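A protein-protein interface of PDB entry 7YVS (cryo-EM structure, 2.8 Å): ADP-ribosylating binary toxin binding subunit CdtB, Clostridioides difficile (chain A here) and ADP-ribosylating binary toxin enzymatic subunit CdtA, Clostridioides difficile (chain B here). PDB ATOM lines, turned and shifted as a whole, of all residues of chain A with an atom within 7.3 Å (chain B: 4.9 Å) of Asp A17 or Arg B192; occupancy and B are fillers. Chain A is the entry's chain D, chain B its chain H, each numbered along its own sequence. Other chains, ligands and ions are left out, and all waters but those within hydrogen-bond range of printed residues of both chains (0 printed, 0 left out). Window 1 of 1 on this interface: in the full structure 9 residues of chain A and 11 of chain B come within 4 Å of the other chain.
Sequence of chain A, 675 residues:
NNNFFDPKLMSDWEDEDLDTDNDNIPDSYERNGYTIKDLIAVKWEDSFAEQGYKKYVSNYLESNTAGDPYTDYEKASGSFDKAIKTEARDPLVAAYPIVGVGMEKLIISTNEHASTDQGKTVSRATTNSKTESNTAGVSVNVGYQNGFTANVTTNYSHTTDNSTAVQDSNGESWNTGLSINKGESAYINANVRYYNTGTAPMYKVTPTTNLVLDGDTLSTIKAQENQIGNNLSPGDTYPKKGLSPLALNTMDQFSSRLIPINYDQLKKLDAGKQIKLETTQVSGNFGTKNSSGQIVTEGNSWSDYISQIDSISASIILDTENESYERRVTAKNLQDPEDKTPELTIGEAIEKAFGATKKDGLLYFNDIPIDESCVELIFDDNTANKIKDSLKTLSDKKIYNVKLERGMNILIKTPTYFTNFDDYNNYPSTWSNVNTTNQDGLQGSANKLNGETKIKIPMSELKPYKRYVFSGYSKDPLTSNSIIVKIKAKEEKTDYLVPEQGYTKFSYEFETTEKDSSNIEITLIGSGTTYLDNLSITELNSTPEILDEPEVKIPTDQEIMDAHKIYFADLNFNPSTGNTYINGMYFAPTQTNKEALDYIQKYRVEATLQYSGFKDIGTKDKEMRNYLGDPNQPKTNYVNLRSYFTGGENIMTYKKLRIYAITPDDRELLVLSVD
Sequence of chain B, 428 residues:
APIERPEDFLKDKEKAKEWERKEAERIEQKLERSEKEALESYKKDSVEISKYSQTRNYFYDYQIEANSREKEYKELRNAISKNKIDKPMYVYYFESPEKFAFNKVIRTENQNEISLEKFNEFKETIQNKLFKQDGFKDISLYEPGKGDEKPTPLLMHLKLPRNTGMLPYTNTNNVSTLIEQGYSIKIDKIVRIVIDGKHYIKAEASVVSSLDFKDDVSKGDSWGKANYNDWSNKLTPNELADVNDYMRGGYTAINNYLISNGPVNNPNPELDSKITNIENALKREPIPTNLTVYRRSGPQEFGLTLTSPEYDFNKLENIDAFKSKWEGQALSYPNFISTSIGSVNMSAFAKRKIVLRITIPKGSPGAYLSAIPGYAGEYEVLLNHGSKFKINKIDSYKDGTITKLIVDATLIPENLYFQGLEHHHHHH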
ATOM      1  N   TRP A  13      18.634  12.450  -9.988  1.00  0.00           N
ATOM      2  CA  TRP A  13      18.367  12.246  -8.570  1.00  0.00           C
ATOM      3  C   TRP A  13      19.156  11.123  -7.907  1.00  0.00           C
ATOM      4  O   TRP A  13      20.185  10.674  -8.405  1.00  0.00           O
ATOM      5  CB  TRP A  13      16.892  11.967  -8.344  1.00  0.00           C
ATOM      6  CG  TRP A  13      16.401  10.862  -9.176  1.00  0.00           C
ATOM      7  CD1 TRP A  13      16.586   9.530  -8.969  1.00  0.00           C
ATOM      8  CD2 TRP A  13      15.522  10.976 -10.289  1.00  0.00           C
ATOM      9  NE1 TRP A  13      15.938   8.807  -9.936  1.00  0.00           N
ATOM     10  CE2 TRP A  13      15.265   9.675 -10.753  1.00  0.00           C
ATOM     11  CE3 TRP A  13      14.947  12.055 -10.955  1.00  0.00           C
ATOM     12  CZ2 TRP A  13      14.463   9.425 -11.851  1.00  0.00           C
ATOM     13  CZ3 TRP A  13      14.149  11.807 -12.037  1.00  0.00           C
ATOM     14  CH2 TRP A  13      13.913  10.502 -12.480  1.00  0.00           C
ATOM     15  N   GLU A  14      18.631  10.677  -6.770  1.00  0.00           N
ATOM     16  CA  GLU A  14      19.346   9.787  -5.859  1.00  0.00           C
ATOM     17  C   GLU A  14      18.956   8.328  -6.089  1.00  0.00           C
ATOM     18  O   GLU A  14      18.357   7.679  -5.230  1.00  0.00           O
ATOM     19  CB  GLU A  14      19.087  10.204  -4.414  1.00  0.00           C
ATOM     20  CG  GLU A  14      19.519  11.626  -4.099  1.00  0.00           C
ATOM     21  CD  GLU A  14      18.395  12.624  -4.279  1.00  0.00           C
ATOM     22  OE1 GLU A  14      17.232  12.267  -3.998  1.00  0.00           O
ATOM     23  OE2 GLU A  14      18.669  13.763  -4.706  1.00  0.00           O
ATOM     24  N   ASP A  15      19.309   7.820  -7.268  1.00  0.00           N
ATOM     25  CA  ASP A  15      19.234   6.395  -7.570  1.00  0.00           C
ATOM     26  C   ASP A  15      19.874   6.164  -8.928  1.00  0.00           C
ATOM     27  O   ASP A  15      19.921   7.065  -9.769  1.00  0.00           O
ATOM     28  CB  ASP A  15      17.795   5.873  -7.562  1.00  0.00           C
ATOM     29  CG  ASP A  15      17.723   4.379  -7.321  1.00  0.00           C
ATOM     30  OD1 ASP A  15      18.791   3.746  -7.210  1.00  0.00           O
ATOM     31  OD2 ASP A  15      16.603   3.837  -7.238  1.00  0.00           O
ATOM     32  N   GLU A  16      20.360   4.945  -9.138  1.00  0.00           N
ATOM     33  CA  GLU A  16      21.015   4.591 -10.397  1.00  0.00           C
ATOM     34  C   GLU A  16      20.012   4.101 -11.438  1.00  0.00           C
ATOM     35  O   GLU A  16      20.145   3.024 -12.019  1.00  0.00           O
ATOM     36  CB  GLU A  16      22.101   3.555 -10.144  1.00  0.00           C
ATOM     37  CG  GLU A  16      23.347   4.137  -9.512  1.00  0.00           C
ATOM     38  CD  GLU A  16      23.294   4.135  -8.001  1.00  0.00           C
ATOM     39  OE1 GLU A  16      22.181   4.048  -7.443  1.00  0.00           O
ATOM     40  OE2 GLU A  16      24.367   4.228  -7.371  1.00  0.00           O
ATOM     41  N   ASP A  17      18.990   4.917 -11.670  1.00  0.00           N
ATOM     42  CA  ASP A  17      17.987   4.707 -12.704  1.00  0.00           C
ATOM     43  C   ASP A  17      17.871   5.947 -13.575  1.00  0.00           C
ATOM     44  O   ASP A  17      16.774   6.414 -13.888  1.00  0.00           O
ATOM     45  CB  ASP A  17      16.641   4.334 -12.092  1.00  0.00           C
ATOM     46  CG  ASP A  17      16.276   5.211 -10.916  1.00  0.00           C
ATOM     47  OD1 ASP A  17      16.876   6.295 -10.770  1.00  0.00           O
ATOM     48  OD2 ASP A  17      15.400   4.808 -10.124  1.00  0.00           O
ATOM     49  N   LEU A  18      19.016   6.505 -13.957  1.00  0.00           N
ATOM     50  CA  LEU A  18      19.102   7.636 -14.867  1.00  0.00           C
ATOM     51  C   LEU A  18      19.902   7.220 -16.088  1.00  0.00           C
ATOM     52  O   LEU A  18      20.936   6.559 -15.960  1.00  0.00           O
ATOM     53  CB  LEU A  18      19.770   8.840 -14.200  1.00  0.00           C
ATOM     54  CG  LEU A  18      19.053   9.555 -13.059  1.00  0.00           C
ATOM     55  CD1 LEU A  18      19.954  10.610 -12.475  1.00  0.00           C
ATOM     56  CD2 LEU A  18      17.775  10.180 -13.557  1.00  0.00           C
ATOM     57  N   ASP A  19      19.417   7.594 -17.270  1.00  0.00           N
ATOM     58  CA  ASP A  19      20.141   7.416 -18.527  1.00  0.00           C
ATOM     59  C   ASP A  19      19.912   8.681 -19.346  1.00  0.00           C
ATOM     60  O   ASP A  19      18.970   8.751 -20.135  1.00  0.00           O
ATOM     61  CB  ASP A  19      19.669   6.173 -19.255  1.00  0.00           C
ATOM     62  CG  ASP A  19      20.668   5.679 -20.266  1.00  0.00           C
ATOM     63  OD1 ASP A  19      21.776   6.247 -20.334  1.00  0.00           O
ATOM     64  OD2 ASP A  19      20.345   4.723 -20.996  1.00  0.00           O
ATOM     65  N   THR A  20      20.784   9.673 -19.168  1.00  0.00           N
ATOM     66  CA  THR A  20      20.541  10.982 -19.766  1.00  0.00           C
ATOM     67  C   THR A  20      20.703  10.945 -21.279  1.00  0.00           C
ATOM     68  O   THR A  20      19.872  11.488 -22.014  1.00  0.00           O
ATOM     69  CB  THR A  20      21.476  12.020 -19.149  1.00  0.00           C
ATOM     70  OG1 THR A  20      21.286  12.047 -17.731  1.00  0.00           O
ATOM     71  CG2 THR A  20      21.185  13.390 -19.712  1.00  0.00           C
ATOM     72  N   ASP A  21      21.767  10.312 -21.768  1.00  0.00           N
ATOM     73  CA  ASP A  21      22.004  10.258 -23.202  1.00  0.00           C
ATOM     74  C   ASP A  21      21.264   9.122 -23.884  1.00  0.00           C
ATOM     75  O   ASP A  21      21.313   9.031 -25.115  1.00  0.00           O
ATOM     76  CB  ASP A  21      23.497  10.130 -23.485  1.00  0.00           C
ATOM     77  CG  ASP A  21      24.158   9.099 -22.617  1.00  0.00           C
ATOM     78  OD1 ASP A  21      23.518   8.639 -21.654  1.00  0.00           O
ATOM     79  OD2 ASP A  21      25.315   8.734 -22.899  1.00  0.00           O
ATOM     80  N   ASN A  22      20.593   8.256 -23.122  1.00  0.00           N
ATOM     81  CA  ASN A  22      19.769   7.179 -23.665  1.00  0.00           C
ATOM     82  C   ASN A  22      20.603   6.228 -24.528  1.00  0.00           C
ATOM     83  O   ASN A  22      20.358   6.044 -25.720  1.00  0.00           O
ATOM     84  CB  ASN A  22      18.585   7.757 -24.446  1.00  0.00           C
ATOM     85  CG  ASN A  22      17.588   6.702 -24.866  1.00  0.00           C
ATOM     86  OD1 ASN A  22      17.448   5.667 -24.220  1.00  0.00           O
ATOM     87  ND2 ASN A  22      16.886   6.960 -25.959  1.00  0.00           N
ATOM     88  N   PRO A  26      23.745   3.397 -17.390  1.00  0.00           N
ATOM     89  CA  PRO A  26      23.398   4.431 -16.411  1.00  0.00           C
ATOM     90  C   PRO A  26      24.498   5.472 -16.285  1.00  0.00           C
ATOM     91  O   PRO A  26      25.665   5.216 -16.581  1.00  0.00           O
ATOM     92  CB  PRO A  26      23.222   3.643 -15.111  1.00  0.00           C
ATOM     93  CG  PRO A  26      22.916   2.265 -15.552  1.00  0.00           C
ATOM     94  CD  PRO A  26      23.695   2.051 -16.802  1.00  0.00           C
ATOM     95  N   ASP A  27      24.102   6.669 -15.850  1.00  0.00           N
ATOM     96  CA  ASP A  27      25.031   7.791 -15.802  1.00  0.00           C
ATOM     97  C   ASP A  27      26.188   7.515 -14.852  1.00  0.00           C
ATOM     98  O   ASP A  27      27.350   7.784 -15.175  1.00  0.00           O
ATOM     99  CB  ASP A  27      24.289   9.060 -15.390  1.00  0.00           C
ATOM    100  CG  ASP A  27      23.397   9.591 -16.486  1.00  0.00           C
ATOM    101  OD1 ASP A  27      23.473   9.073 -17.617  1.00  0.00           O
ATOM    102  OD2 ASP A  27      22.624  10.532 -16.218  1.00  0.00           O
ATOM    103  N   SER A  28      25.890   6.977 -13.667  1.00  0.00           N
ATOM    104  CA  SER A  28      26.948   6.727 -12.695  1.00  0.00           C
ATOM    105  C   SER A  28      27.867   5.601 -13.138  1.00  0.00           C
ATOM    106  O   SER A  28      29.060   5.621 -12.821  1.00  0.00           O
ATOM    107  CB  SER A  28      26.350   6.405 -11.332  1.00  0.00           C
ATOM    108  OG  SER A  28      25.628   5.195 -11.385  1.00  0.00           O
ATOM    109  N   GLU B 113      10.950  19.255 -17.091  1.00  0.00           N
ATOM    110  CA  GLU B 113      11.622  18.392 -16.136  1.00  0.00           C
ATOM    111  C   GLU B 113      10.617  17.503 -15.414  1.00  0.00           C
ATOM    112  O   GLU B 113       9.474  17.892 -15.169  1.00  0.00           O
ATOM    113  CB  GLU B 113      12.416  19.226 -15.123  1.00  0.00           C
ATOM    114  CG  GLU B 113      13.227  18.411 -14.138  1.00  0.00           C
ATOM    115  CD  GLU B 113      14.034  19.275 -13.197  1.00  0.00           C
ATOM    116  OE1 GLU B 113      13.943  20.516 -13.304  1.00  0.00           O
ATOM    117  OE2 GLU B 113      14.760  18.712 -12.352  1.00  0.00           O
ATOM    118  N   ILE B 114      11.064  16.294 -15.079  1.00  0.00           N
ATOM    119  CA  ILE B 114      10.287  15.335 -14.304  1.00  0.00           C
ATOM    120  C   ILE B 114      10.881  15.262 -12.906  1.00  0.00           C
ATOM    121  O   ILE B 114      12.093  15.085 -12.750  1.00  0.00           O
ATOM    122  CB  ILE B 114      10.273  13.945 -14.966  1.00  0.00           C
ATOM    123  CG1 ILE B 114       9.321  13.936 -16.161  1.00  0.00           C
ATOM    124  CG2 ILE B 114       9.879  12.878 -13.965  1.00  0.00           C
ATOM    125  CD1 ILE B 114       9.467  12.728 -17.042  1.00  0.00           C
ATOM    126  N   PHE B 119       8.502  10.304 -10.531  1.00  0.00           N
ATOM    127  CA  PHE B 119       9.140   9.078 -10.992  1.00  0.00           C
ATOM    128  C   PHE B 119       8.890   7.936 -10.019  1.00  0.00           C
ATOM    129  O   PHE B 119       8.527   6.826 -10.428  1.00  0.00           O
ATOM    130  CB  PHE B 119      10.638   9.317 -11.175  1.00  0.00           C
ATOM    131  CG  PHE B 119      11.376   8.150 -11.755  1.00  0.00           C
ATOM    132  CD1 PHE B 119      11.474   7.992 -13.123  1.00  0.00           C
ATOM    133  CD2 PHE B 119      11.989   7.222 -10.932  1.00  0.00           C
ATOM    134  CE1 PHE B 119      12.152   6.924 -13.657  1.00  0.00           C
ATOM    135  CE2 PHE B 119      12.669   6.154 -11.465  1.00  0.00           C
ATOM    136  CZ  PHE B 119      12.751   6.005 -12.827  1.00  0.00           C
ATOM    137  N   LYS B 123       6.729   4.528 -10.382  1.00  0.00           N
ATOM    138  CA  LYS B 123       7.431   3.262 -10.204  1.00  0.00           C
ATOM    139  C   LYS B 123       6.647   2.302  -9.316  1.00  0.00           C
ATOM    140  O   LYS B 123       6.457   1.137  -9.677  1.00  0.00           O
ATOM    141  CB  LYS B 123       8.826   3.511  -9.631  1.00  0.00           C
ATOM    142  CG  LYS B 123       9.733   2.298  -9.687  1.00  0.00           C
ATOM    143  CD  LYS B 123      11.194   2.698  -9.751  1.00  0.00           C
ATOM    144  CE  LYS B 123      11.746   2.982  -8.370  1.00  0.00           C
ATOM    145  NZ  LYS B 123      13.186   3.353  -8.416  1.00  0.00           N
ATOM    146  N   ILE B 190      12.369   1.102 -15.794  1.00  0.00           N
ATOM    147  CA  ILE B 190      12.089   2.454 -16.258  1.00  0.00           C
ATOM    148  C   ILE B 190      13.255   3.358 -15.880  1.00  0.00           C
ATOM    149  O   ILE B 190      13.802   3.253 -14.778  1.00  0.00           O
ATOM    150  CB  ILE B 190      10.767   3.000 -15.679  1.00  0.00           C
ATOM    151  CG1 ILE B 190      10.730   2.844 -14.162  1.00  0.00           C
ATOM    152  CG2 ILE B 190       9.584   2.290 -16.294  1.00  0.00           C
ATOM    153  CD1 ILE B 190       9.724   3.746 -13.495  1.00  0.00           C
ATOM    154  N   VAL B 191      13.648   4.233 -16.806  1.00  0.00           N
ATOM    155  CA  VAL B 191      14.689   5.225 -16.577  1.00  0.00           C
ATOM    156  C   VAL B 191      14.204   6.562 -17.119  1.00  0.00           C
ATOM    157  O   VAL B 191      13.265   6.633 -17.913  1.00  0.00           O
ATOM    158  CB  VAL B 191      16.034   4.842 -17.233  1.00  0.00           C
ATOM    159  CG1 VAL B 191      16.577   3.557 -16.641  1.00  0.00           C
ATOM    160  CG2 VAL B 191      15.875   4.717 -18.731  1.00  0.00           C
ATOM    161  N   ARG B 192      14.862   7.633 -16.684  1.00  0.00           N
ATOM    162  CA  ARG B 192      14.563   8.976 -17.163  1.00  0.00           C
ATOM    163  C   ARG B 192      15.620   9.417 -18.166  1.00  0.00           C
ATOM    164  O   ARG B 192      16.814   9.408 -17.858  1.00  0.00           O
ATOM    165  CB  ARG B 192      14.490   9.977 -16.011  1.00  0.00           C
ATOM    166  CG  ARG B 192      14.088  11.371 -16.459  1.00  0.00           C
ATOM    167  CD  ARG B 192      14.212  12.373 -15.338  1.00  0.00           C
ATOM    168  NE  ARG B 192      15.601  12.707 -15.045  1.00  0.00           N
ATOM    169  CZ  ARG B 192      15.983  13.668 -14.215  1.00  0.00           C
ATOM    170  NH1 ARG B 192      15.104  14.408 -13.565  1.00  0.00           N
ATOM    171  NH2 ARG B 192      17.280  13.884 -14.026  1.00  0.00           N
ATOM    172  N   ILE B 193      15.172   9.815 -19.355  1.00  0.00           N
ATOM    173  CA  ILE B 193      16.051  10.190 -20.451  1.00  0.00           C
ATOM    174  C   ILE B 193      15.744  11.626 -20.862  1.00  0.00           C
ATOM    175  O   ILE B 193      14.755  12.221 -20.439  1.00  0.00           O
ATOM    176  CB  ILE B 193      15.915   9.239 -21.654  1.00  0.00           C
ATOM    177  CG1 ILE B 193      14.557   9.430 -22.328  1.00  0.00           C
ATOM    178  CG2 ILE B 193      16.090   7.802 -21.214  1.00  0.00           C
ATOM    179  CD1 ILE B 193      14.368   8.611 -23.567  1.00  0.00           C
ATOM    180  N   VAL B 194      16.617  12.180 -21.697  1.00  0.00           N
ATOM    181  CA  VAL B 194      16.477  13.534 -22.219  1.00  0.00           C
ATOM    182  C   VAL B 194      16.389  13.454 -23.734  1.00  0.00           C
ATOM    183  O   VAL B 194      17.257  12.855 -24.378  1.00  0.00           O
ATOM    184  CB  VAL B 194      17.653  14.434 -21.794  1.00  0.00           C
ATOM    185  CG1 VAL B 194      17.603  15.762 -22.525  1.00  0.00           C
ATOM    186  CG2 VAL B 194      17.652  14.650 -20.295  1.00  0.00           C
ATOM    187  N   HIS B 199      12.570  15.993 -20.390  1.00  0.00           N
ATOM    188  CA  HIS B 199      12.683  14.725 -19.685  1.00  0.00           C
ATOM    189  C   HIS B 199      11.563  13.778 -20.094  1.00  0.00           C
ATOM    190  O   HIS B 199      10.401  14.176 -20.203  1.00  0.00           O
ATOM    191  CB  HIS B 199      12.643  14.950 -18.176  1.00  0.00           C
ATOM    192  CG  HIS B 199      13.936  15.436 -17.603  1.00  0.00           C
ATOM    193  ND1 HIS B 199      14.029  15.990 -16.345  1.00  0.00           N
ATOM    194  CD2 HIS B 199      15.188  15.445 -18.111  1.00  0.00           C
ATOM    195  CE1 HIS B 199      15.283  16.325 -16.107  1.00  0.00           C
ATOM    196  NE2 HIS B 199      16.006  16.005 -17.164  1.00  0.00           N
ATOM    197  N   TYR B 200      11.921  12.517 -20.314  1.00  0.00           N
ATOM    198  CA  TYR B 200      10.966  11.471 -20.641  1.00  0.00           C
ATOM    199  C   TYR B 200      11.233  10.261 -19.762  1.00  0.00           C
ATOM    200  O   TYR B 200      12.349  10.048 -19.287  1.00  0.00           O
ATOM    201  CB  TYR B 200      11.050  11.057 -22.116  1.00  0.00           C
ATOM    202  CG  TYR B 200      10.568  12.106 -23.082  1.00  0.00           C
ATOM    203  CD1 TYR B 200      11.405  13.130 -23.491  1.00  0.00           C
ATOM    204  CD2 TYR B 200       9.283  12.067 -23.594  1.00  0.00           C
ATOM    205  CE1 TYR B 200      10.973  14.088 -24.373  1.00  0.00           C
ATOM    206  CE2 TYR B 200       8.843  13.023 -24.479  1.00  0.00           C
ATOM    207  CZ  TYR B 200       9.694  14.030 -24.863  1.00  0.00           C
ATOM    208  OH  TYR B 200       9.267  14.990 -25.746  1.00  0.00           O
ATOM    209  N   ILE B 201      10.192   9.466 -19.550  1.00  0.00           N
ATOM    210  CA  ILE B 201      10.296   8.202 -18.832  1.00  0.00           C
ATOM    211  C   ILE B 201      10.268   7.089 -19.865  1.00  0.00           C
ATOM    212  O   ILE B 201       9.291   6.948 -20.609  1.00  0.00           O
ATOM    213  CB  ILE B 201       9.169   8.033 -17.804  1.00  0.00           C
ATOM    214  CG1 ILE B 201       9.326   9.045 -16.671  1.00  0.00           C
ATOM    215  CG2 ILE B 201       9.162   6.621 -17.259  1.00  0.00           C
ATOM    216  CD1 ILE B 201       8.330   8.866 -15.560  1.00  0.00           C
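The side-chain amino group of Lys B123 is in salt-bridge range of the side-chain carboxylate of Asp A15, at 3.6 Å. OD2 of Asp A17 is in salt-bridge range of NZ of Lys B123 (3.2 Å). N of Asp A19 is in hydrogen-bond range of O of Arg B192, 3.2 Å away. The backbone NH (N) of Val B194 lies within hydrogen-bond range of the backbone carbonyl oxygen (O) of Thr A20 (3.3 Å).
Of chain B, only Phe B119, Lys B123, Val B191 and Arg B192 come within 4 Å of Asp A17. Printed residues of chain B within 4 Å of Thr A20: Val B194 (3.3 Å). Pro A26 touches none of the printed residues of chain B. Asp A27 touches none of the printed residues of chain B. Of the printed residues of chain A, Ile B114 touches Trp A13. Of chain A, only Trp A13, Asp A17, Leu A18 and Asp A19 come within 4 Å of Arg B192. Of the printed residues of chain A, Val B194 touches Thr A20 (3.3 Å). The nearest residue of chain B that does not touch Asp A17 is Ile B190 (4.1 Å). The nearest printed residue of chain A that does not touch Ile B114 is Leu A18 (7.5 Å).
Among the printed residues, pairs that only touch across the chains: Trp A13 with Arg B192 (3.2 Å), Asp A19 with Ile B193 (3.2 Å), Asp A17 with Phe B119 (3.3 Å), Trp A13 with Phe B119 (3.3 Å), Asp A17 with Arg B192 (3.6 Å), Asp A17 with Val B191 (3.6 Å), Leu A18 with Arg B192 (3.7 Å), Asn A22 with Ile B193 (3.8 Å) and Trp A13 with Ile B114 (3.9 Å).
Printed residues of chain A that touch a printed residue of chain B: Trp A13, Asp A15, Asp A17, Leu A18, Asp A19, Thr A20 and Asn A22. Hydrophobic or aromatic side chains of chain B within 4 Å of the printed part of chain A: Phe B119, Val B191, Ile B193 and Val B194. Among the printed residues, 13 pairs touch across the chains.
NE1 of Trp A13 lies within hydrogen-bond range of OD1 of Asp A17, at 2.8 Å. O of Leu A18 is in hydrogen-bond range of N of Asp A27 (3.2 Å). The side-chain hydroxyl (OG1) of Thr A20 is in hydrogen-bond range of the side-chain carboxylate (OD2) of Asp A27, 2.5 Å away. O of Ile B114 lies within hydrogen-bond range of NH1 of Arg B192 (3.2 Å). ND1 of His B199 sits close to NH1 of Arg B192. The backbone NH (N) of Ile B193 sits at hydrogen-bond distance from the backbone carbonyl oxygen (O) of Tyr B200 (2.8 Å).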
